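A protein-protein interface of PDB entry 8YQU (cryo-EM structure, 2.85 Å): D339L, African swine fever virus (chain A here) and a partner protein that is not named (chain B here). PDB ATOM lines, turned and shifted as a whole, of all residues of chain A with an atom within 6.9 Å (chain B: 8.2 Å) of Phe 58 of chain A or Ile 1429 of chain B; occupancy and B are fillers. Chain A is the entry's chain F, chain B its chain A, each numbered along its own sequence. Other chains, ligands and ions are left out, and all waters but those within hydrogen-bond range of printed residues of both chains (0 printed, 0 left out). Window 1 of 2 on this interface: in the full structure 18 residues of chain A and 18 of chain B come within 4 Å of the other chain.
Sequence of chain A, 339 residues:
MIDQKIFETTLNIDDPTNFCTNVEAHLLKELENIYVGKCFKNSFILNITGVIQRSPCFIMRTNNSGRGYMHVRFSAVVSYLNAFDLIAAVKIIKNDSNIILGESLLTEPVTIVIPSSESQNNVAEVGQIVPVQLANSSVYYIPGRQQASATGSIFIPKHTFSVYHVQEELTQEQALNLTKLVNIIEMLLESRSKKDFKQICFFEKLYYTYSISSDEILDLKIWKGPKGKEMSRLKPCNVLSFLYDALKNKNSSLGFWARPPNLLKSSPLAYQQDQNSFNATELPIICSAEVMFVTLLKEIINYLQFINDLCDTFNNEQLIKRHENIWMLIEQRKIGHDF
Printed residues of chain B within 4 Å of Cys 57 of chain A: Ile 1430 and Met 1431.
Phe 58 of chain A touches just these residues of chain B: Ile 1429 (3.8 Å) and Ile 1430 (3.5 Å).
Printed residues of chain B within 4 Å of Met 60 of chain A: Tyr 5 (3.6 Å).
Printed residues of chain A within 4 Å of Tyr 5 of chain B: Met 60 and Tyr 69.
Ile 1429 of chain B touches just these residues of chain A: Phe 58 (3.8 Å) and Ile 59 (3.0 Å).
The backbone carbonyl oxygen of Cys 57 of chain A is in hydrogen-bond range of the backbone NH of Met 1431 of chain B (2.8 Å).
O of Ile 1429 of chain B is in hydrogen-bond range of N of Ile 59 of chain A (3.0 Å).
Of the 14 printed residues of chain A, 7 touch a printed residue of chain B.
Hydrophobic or aromatic side chains of chain A within 4 Å of the printed part of chain B: Pro 16, Pro 56, Phe 58, Ile 59, Met 60 and Tyr 69.
Of the 10 printed residues of chain B, 4 touch a printed residue of chain A.
Hydrophobic or aromatic side chains of chain B that line the printed part of chain A: Tyr 5, Ile 1430 and Met 1431.
Among the printed residues, 10 pairs touch across the chains.
Among the printed residues, merely in contact across the chains: Pro 16 of chain A with Met 1431 of chain B (3.5 Å), Pro 56 of chain A with Ile 1430 of chain B (3.98 Å), Cys 57 of chain A with Ile 1430 of chain B (3.5 Å), Phe 58 of chain A with Ile 1429 of chain B (3.8 Å), Phe 58 of chain A with Ile 1430 of chain B (3.5 Å), Ile 59 of chain A with Met 1431 of chain B (3.7 Å), Met 60 of chain A with Tyr 5 of chain B (3.6 Å) and Tyr 69 of chain A with Tyr 5 of chain B (3.4 Å).
The backbone carbonyl oxygen of Arg 67 of chain A lies within hydrogen-bond range of the backbone NH of Met 60 of chain A (3.0 Å).
The backbone carbonyl oxygen (O) of Tyr 69 of chain A is in hydrogen-bond range of the backbone NH (N) of Phe 58 of chain A (3.0 Å).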
ATOM      1  N   ILE A  13       3.495   2.662  -3.422  1.00  0.00           N
ATOM      2  CA  ILE A  13       4.288   3.695  -4.074  1.00  0.00           C
ATOM      3  C   ILE A  13       3.669   3.975  -5.435  1.00  0.00           C
ATOM      4  O   ILE A  13       3.736   3.132  -6.340  1.00  0.00           O
ATOM      5  CB  ILE A  13       5.758   3.278  -4.220  1.00  0.00           C
ATOM      6  CG1 ILE A  13       6.429   3.115  -2.851  1.00  0.00           C
ATOM      7  CG2 ILE A  13       6.490   4.270  -5.087  1.00  0.00           C
ATOM      8  CD1 ILE A  13       6.324   1.724  -2.265  1.00  0.00           C
ATOM      9  N   PRO A  16       7.096   4.542  -8.740  1.00  0.00           N
ATOM     10  CA  PRO A  16       8.328   3.893  -8.265  1.00  0.00           C
ATOM     11  C   PRO A  16       9.605   4.585  -8.709  1.00  0.00           C
ATOM     12  O   PRO A  16      10.592   4.575  -7.962  1.00  0.00           O
ATOM     13  CB  PRO A  16       8.220   2.479  -8.853  1.00  0.00           C
ATOM     14  CG  PRO A  16       6.764   2.290  -9.139  1.00  0.00           C
ATOM     15  CD  PRO A  16       6.274   3.636  -9.557  1.00  0.00           C
ATOM     16  N   SER A  55      11.723  -4.248   2.179  1.00  0.00           N
ATOM     17  CA  SER A  55      11.703  -5.108   1.008  1.00  0.00           C
ATOM     18  C   SER A  55      12.110  -4.334  -0.236  1.00  0.00           C
ATOM     19  O   SER A  55      12.065  -3.100  -0.258  1.00  0.00           O
ATOM     20  CB  SER A  55      10.307  -5.693   0.815  1.00  0.00           C
ATOM     21  OG  SER A  55       9.425  -4.739   0.253  1.00  0.00           O
ATOM     22  N   PRO A  56      12.527  -5.032  -1.292  1.00  0.00           N
ATOM     23  CA  PRO A  56      12.699  -4.363  -2.584  1.00  0.00           C
ATOM     24  C   PRO A  56      11.371  -3.812  -3.075  1.00  0.00           C
ATOM     25  O   PRO A  56      10.302  -4.341  -2.767  1.00  0.00           O
ATOM     26  CB  PRO A  56      13.215  -5.479  -3.499  1.00  0.00           C
ATOM     27  CG  PRO A  56      13.798  -6.491  -2.578  1.00  0.00           C
ATOM     28  CD  PRO A  56      12.977  -6.434  -1.329  1.00  0.00           C
ATOM     29  N   CYS A  57      11.443  -2.726  -3.842  1.00  0.00           N
ATOM     30  CA  CYS A  57      10.224  -2.113  -4.352  1.00  0.00           C
ATOM     31  C   CYS A  57       9.610  -2.990  -5.435  1.00  0.00           C
ATOM     32  O   CYS A  57       9.976  -2.885  -6.610  1.00  0.00           O
ATOM     33  CB  CYS A  57      10.506  -0.711  -4.894  1.00  0.00           C
ATOM     34  SG  CYS A  57       9.050   0.133  -5.553  1.00  0.00           S
ATOM     35  N   PHE A  58       8.683  -3.861  -5.047  1.00  0.00           N
ATOM     36  CA  PHE A  58       8.031  -4.732  -6.010  1.00  0.00           C
ATOM     37  C   PHE A  58       7.056  -3.936  -6.872  1.00  0.00           C
ATOM     38  O   PHE A  58       6.668  -2.810  -6.551  1.00  0.00           O
ATOM     39  CB  PHE A  58       7.286  -5.863  -5.303  1.00  0.00           C
ATOM     40  CG  PHE A  58       8.144  -6.689  -4.390  1.00  0.00           C
ATOM     41  CD1 PHE A  58       8.958  -7.685  -4.896  1.00  0.00           C
ATOM     42  CD2 PHE A  58       8.115  -6.485  -3.022  1.00  0.00           C
ATOM     43  CE1 PHE A  58       9.742  -8.449  -4.058  1.00  0.00           C
ATOM     44  CE2 PHE A  58       8.896  -7.248  -2.179  1.00  0.00           C
ATOM     45  CZ  PHE A  58       9.710  -8.231  -2.698  1.00  0.00           C
ATOM     46  N   ILE A  59       6.659  -4.543  -7.986  1.00  0.00           N
ATOM     47  CA  ILE A  59       5.622  -4.009  -8.860  1.00  0.00           C
ATOM     48  C   ILE A  59       4.373  -4.854  -8.661  1.00  0.00           C
ATOM     49  O   ILE A  59       4.439  -6.088  -8.716  1.00  0.00           O
ATOM     50  CB  ILE A  59       6.064  -4.012 -10.334  1.00  0.00           C
ATOM     51  CG1 ILE A  59       7.353  -3.209 -10.505  1.00  0.00           C
ATOM     52  CG2 ILE A  59       4.967  -3.448 -11.219  1.00  0.00           C
ATOM     53  CD1 ILE A  59       7.247  -1.782 -10.033  1.00  0.00           C
ATOM     54  N   MET A  60       3.244  -4.194  -8.413  1.00  0.00           N
ATOM     55  CA  MET A  60       2.003  -4.909  -8.148  1.00  0.00           C
ATOM     56  C   MET A  60       1.635  -5.805  -9.324  1.00  0.00           C
ATOM     57  O   MET A  60       1.714  -5.398 -10.486  1.00  0.00           O
ATOM     58  CB  MET A  60       0.878  -3.923  -7.844  1.00  0.00           C
ATOM     59  CG  MET A  60       1.331  -2.732  -7.024  1.00  0.00           C
ATOM     60  SD  MET A  60       0.018  -2.015  -6.027  1.00  0.00           S
ATOM     61  CE  MET A  60      -1.235  -1.802  -7.278  1.00  0.00           C
ATOM     62  N   GLY A  66       0.900  -0.519 -13.078  1.00  0.00           N
ATOM     63  CA  GLY A  66       2.324  -0.261 -13.016  1.00  0.00           C
ATOM     64  C   GLY A  66       2.795   0.348 -11.718  1.00  0.00           C
ATOM     65  O   GLY A  66       3.949   0.777 -11.630  1.00  0.00           O
ATOM     66  N   ARG A  67       1.934   0.396 -10.706  1.00  0.00           N
ATOM     67  CA  ARG A  67       2.250   0.979  -9.415  1.00  0.00           C
ATOM     68  C   ARG A  67       3.054  -0.031  -8.596  1.00  0.00           C
ATOM     69  O   ARG A  67       3.158  -1.207  -8.952  1.00  0.00           O
ATOM     70  CB  ARG A  67       0.950   1.442  -8.749  1.00  0.00           C
ATOM     71  CG  ARG A  67       1.101   2.210  -7.455  1.00  0.00           C
ATOM     72  CD  ARG A  67      -0.222   2.769  -6.935  1.00  0.00           C
ATOM     73  NE  ARG A  67      -1.205   1.763  -6.556  1.00  0.00           N
ATOM     74  CZ  ARG A  67      -2.364   1.589  -7.175  1.00  0.00           C
ATOM     75  NH1 ARG A  67      -2.701   2.316  -8.228  1.00  0.00           N
ATOM     76  NH2 ARG A  67      -3.212   0.672  -6.720  1.00  0.00           N
ATOM     77  N   GLY A  68       3.675   0.426  -7.504  1.00  0.00           N
ATOM     78  CA  GLY A  68       4.570  -0.402  -6.727  1.00  0.00           C
ATOM     79  C   GLY A  68       4.145  -0.524  -5.270  1.00  0.00           C
ATOM     80  O   GLY A  68       3.241   0.170  -4.800  1.00  0.00           O
ATOM     81  N   TYR A  69       4.829  -1.414  -4.554  1.00  0.00           N
ATOM     82  CA  TYR A  69       4.599  -1.571  -3.125  1.00  0.00           C
ATOM     83  C   TYR A  69       5.882  -2.045  -2.459  1.00  0.00           C
ATOM     84  O   TYR A  69       6.763  -2.614  -3.107  1.00  0.00           O
ATOM     85  CB  TYR A  69       3.454  -2.550  -2.837  1.00  0.00           C
ATOM     86  CG  TYR A  69       3.727  -3.976  -3.253  1.00  0.00           C
ATOM     87  CD1 TYR A  69       3.537  -4.386  -4.565  1.00  0.00           C
ATOM     88  CD2 TYR A  69       4.158  -4.918  -2.329  1.00  0.00           C
ATOM     89  CE1 TYR A  69       3.779  -5.688  -4.947  1.00  0.00           C
ATOM     90  CE2 TYR A  69       4.402  -6.222  -2.702  1.00  0.00           C
ATOM     91  CZ  TYR A  69       4.210  -6.602  -4.012  1.00  0.00           C
ATOM     92  OH  TYR A  69       4.453  -7.901  -4.389  1.00  0.00           O
ATOM     93  N   MET A  70       5.976  -1.799  -1.153  1.00  0.00           N
ATOM     94  CA  MET A  70       7.167  -2.138  -0.385  1.00  0.00           C
ATOM     95  C   MET A  70       6.775  -2.560   1.022  1.00  0.00           C
ATOM     96  O   MET A  70       5.949  -1.903   1.660  1.00  0.00           O
ATOM     97  CB  MET A  70       8.140  -0.952  -0.326  1.00  0.00           C
ATOM     98  CG  MET A  70       9.283  -1.132   0.659  1.00  0.00           C
ATOM     99  SD  MET A  70      10.600   0.082   0.460  1.00  0.00           S
ATOM    100  CE  MET A  70      10.660   0.237  -1.320  1.00  0.00           C
ATOM    101  N   HIS A  71       7.372  -3.648   1.505  1.00  0.00           N
ATOM    102  CA  HIS A  71       7.175  -4.078   2.885  1.00  0.00           C
ATOM    103  C   HIS A  71       8.182  -3.363   3.777  1.00  0.00           C
ATOM    104  O   HIS A  71       9.390  -3.428   3.531  1.00  0.00           O
ATOM    105  CB  HIS A  71       7.331  -5.591   3.006  1.00  0.00           C
ATOM    106  CG  HIS A  71       6.436  -6.369   2.092  1.00  0.00           C
ATOM    107  ND1 HIS A  71       5.062  -6.280   2.141  1.00  0.00           N
ATOM    108  CD2 HIS A  71       6.720  -7.256   1.110  1.00  0.00           C
ATOM    109  CE1 HIS A  71       4.538  -7.074   1.226  1.00  0.00           C
ATOM    110  NE2 HIS A  71       5.522  -7.679   0.586  1.00  0.00           N
ATOM    111  N   TYR B   5      -0.806  -3.140  -0.262  1.00  0.00           N
ATOM    112  CA  TYR B   5      -1.072  -4.143  -1.282  1.00  0.00           C
ATOM    113  C   TYR B   5      -0.820  -5.537  -0.724  1.00  0.00           C
ATOM    114  O   TYR B   5       0.131  -5.757   0.031  1.00  0.00           O
ATOM    115  CB  TYR B   5      -0.193  -3.899  -2.508  1.00  0.00           C
ATOM    116  CG  TYR B   5      -0.336  -4.943  -3.591  1.00  0.00           C
ATOM    117  CD1 TYR B   5      -1.409  -4.917  -4.470  1.00  0.00           C
ATOM    118  CD2 TYR B   5       0.601  -5.955  -3.734  1.00  0.00           C
ATOM    119  CE1 TYR B   5      -1.542  -5.867  -5.461  1.00  0.00           C
ATOM    120  CE2 TYR B   5       0.478  -6.909  -4.722  1.00  0.00           C
ATOM    121  CZ  TYR B   5      -0.596  -6.861  -5.581  1.00  0.00           C
ATOM    122  OH  TYR B   5      -0.723  -7.812  -6.565  1.00  0.00           O
ATOM    123  N   THR B1424       3.552 -14.067 -18.104  1.00  0.00           N
ATOM    124  CA  THR B1424       4.115 -12.769 -17.751  1.00  0.00           C
ATOM    125  C   THR B1424       4.075 -12.528 -16.248  1.00  0.00           C
ATOM    126  O   THR B1424       4.888 -11.757 -15.726  1.00  0.00           O
ATOM    127  CB  THR B1424       3.371 -11.650 -18.479  1.00  0.00           C
ATOM    128  OG1 THR B1424       1.980 -11.701 -18.146  1.00  0.00           O
ATOM    129  CG2 THR B1424       3.530 -11.797 -19.978  1.00  0.00           C
ATOM    130  N   MET B1425       3.150 -13.170 -15.543  1.00  0.00           N
ATOM    131  CA  MET B1425       3.006 -12.989 -14.107  1.00  0.00           C
ATOM    132  C   MET B1425       3.857 -13.961 -13.300  1.00  0.00           C
ATOM    133  O   MET B1425       3.871 -13.871 -12.069  1.00  0.00           O
ATOM    134  CB  MET B1425       1.538 -13.147 -13.700  1.00  0.00           C
ATOM    135  CG  MET B1425       0.593 -12.107 -14.287  1.00  0.00           C
ATOM    136  SD  MET B1425       0.938 -10.400 -13.828  1.00  0.00           S
ATOM    137  CE  MET B1425       1.720  -9.803 -15.321  1.00  0.00           C
ATOM    138  N   TYR B1426       4.557 -14.889 -13.958  1.00  0.00           N
ATOM    139  CA  TYR B1426       5.313 -15.903 -13.230  1.00  0.00           C
ATOM    140  C   TYR B1426       6.476 -15.286 -12.464  1.00  0.00           C
ATOM    141  O   TYR B1426       6.652 -15.546 -11.268  1.00  0.00           O
ATOM    142  CB  TYR B1426       5.815 -16.979 -14.192  1.00  0.00           C
ATOM    143  CG  TYR B1426       6.276 -18.234 -13.493  1.00  0.00           C
ATOM    144  CD1 TYR B1426       5.362 -19.101 -12.914  1.00  0.00           C
ATOM    145  CD2 TYR B1426       7.624 -18.550 -13.406  1.00  0.00           C
ATOM    146  CE1 TYR B1426       5.775 -20.246 -12.270  1.00  0.00           C
ATOM    147  CE2 TYR B1426       8.046 -19.696 -12.764  1.00  0.00           C
ATOM    148  CZ  TYR B1426       7.118 -20.539 -12.198  1.00  0.00           C
ATOM    149  OH  TYR B1426       7.531 -21.682 -11.555  1.00  0.00           O
ATOM    150  N   SER B1427       7.282 -14.472 -13.135  1.00  0.00           N
ATOM    151  CA  SER B1427       8.407 -13.794 -12.508  1.00  0.00           C
ATOM    152  C   SER B1427       8.022 -12.350 -12.226  1.00  0.00           C
ATOM    153  O   SER B1427       7.691 -11.600 -13.150  1.00  0.00           O
ATOM    154  CB  SER B1427       9.646 -13.845 -13.402  1.00  0.00           C
ATOM    155  OG  SER B1427      10.039 -15.180 -13.656  1.00  0.00           O
ATOM    156  N   ASP B1428       8.064 -11.965 -10.956  1.00  0.00           N
ATOM    157  CA  ASP B1428       7.725 -10.602 -10.582  1.00  0.00           C
ATOM    158  C   ASP B1428       8.902  -9.670 -10.841  1.00  0.00           C
ATOM    159  O   ASP B1428      10.054 -10.094 -10.954  1.00  0.00           O
ATOM    160  CB  ASP B1428       7.286 -10.528  -9.118  1.00  0.00           C
ATOM    161  CG  ASP B1428       8.299 -11.128  -8.165  1.00  0.00           C
ATOM    162  OD1 ASP B1428       9.428 -11.442  -8.593  1.00  0.00           O
ATOM    163  OD2 ASP B1428       7.958 -11.287  -6.974  1.00  0.00           O
ATOM    164  N   ILE B1429       8.593  -8.382 -10.945  1.00  0.00           N
ATOM    165  CA  ILE B1429       9.561  -7.363 -11.322  1.00  0.00           C
ATOM    166  C   ILE B1429       9.770  -6.443 -10.130  1.00  0.00           C
ATOM    167  O   ILE B1429       8.800  -5.969  -9.528  1.00  0.00           O
ATOM    168  CB  ILE B1429       9.088  -6.575 -12.555  1.00  0.00           C
ATOM    169  CG1 ILE B1429       8.839  -7.530 -13.723  1.00  0.00           C
ATOM    170  CG2 ILE B1429      10.109  -5.522 -12.938  1.00  0.00           C
ATOM    171  CD1 ILE B1429      10.058  -8.305 -14.153  1.00  0.00           C
ATOM    172  N   ILE B1430      11.029  -6.200  -9.782  1.00  0.00           N
ATOM    173  CA  ILE B1430      11.369  -5.291  -8.697  1.00  0.00           C
ATOM    174  C   ILE B1430      12.079  -4.083  -9.288  1.00  0.00           C
ATOM    175  O   ILE B1430      12.675  -4.153 -10.368  1.00  0.00           O
ATOM    176  CB  ILE B1430      12.240  -5.963  -7.612  1.00  0.00           C
ATOM    177  CG1 ILE B1430      13.656  -6.207  -8.127  1.00  0.00           C
ATOM    178  CG2 ILE B1430      11.618  -7.272  -7.169  1.00  0.00           C
ATOM    179  CD1 ILE B1430      14.625  -6.622  -7.046  1.00  0.00           C
ATOM    180  N   MET B1431      12.001  -2.967  -8.575  1.00  0.00           N
ATOM    181  CA  MET B1431      12.580  -1.723  -9.054  1.00  0.00           C
ATOM    182  C   MET B1431      14.077  -1.704  -8.780  1.00  0.00           C
ATOM    183  O   MET B1431      14.527  -2.042  -7.682  1.00  0.00           O
ATOM    184  CB  MET B1431      11.909  -0.531  -8.372  1.00  0.00           C
ATOM    185  CG  MET B1431      10.516  -0.214  -8.890  1.00  0.00           C
ATOM    186  SD  MET B1431      10.384  -0.003 -10.672  1.00  0.00           S
ATOM    187  CE  MET B1431      11.613   1.259 -10.970  1.00  0.00           C
ATOM    188  N   ASP B1432      14.852  -1.304  -9.785  1.00  0.00           N
ATOM    189  CA  ASP B1432      16.311  -1.278  -9.677  1.00  0.00           C
ATOM    190  C   ASP B1432      16.713  -0.066  -8.847  1.00  0.00           C
ATOM    191  O   ASP B1432      16.861   1.046  -9.355  1.00  0.00           O
ATOM    192  CB  ASP B1432      16.952  -1.253 -11.057  1.00  0.00           C
ATOM    193  CG  ASP B1432      18.365  -1.795 -11.049  1.00  0.00           C
ATOM    194  OD1 ASP B1432      18.914  -2.013  -9.949  1.00  0.00           O
ATOM    195  OD2 ASP B1432      18.924  -2.011 -12.143  1.00  0.00           O
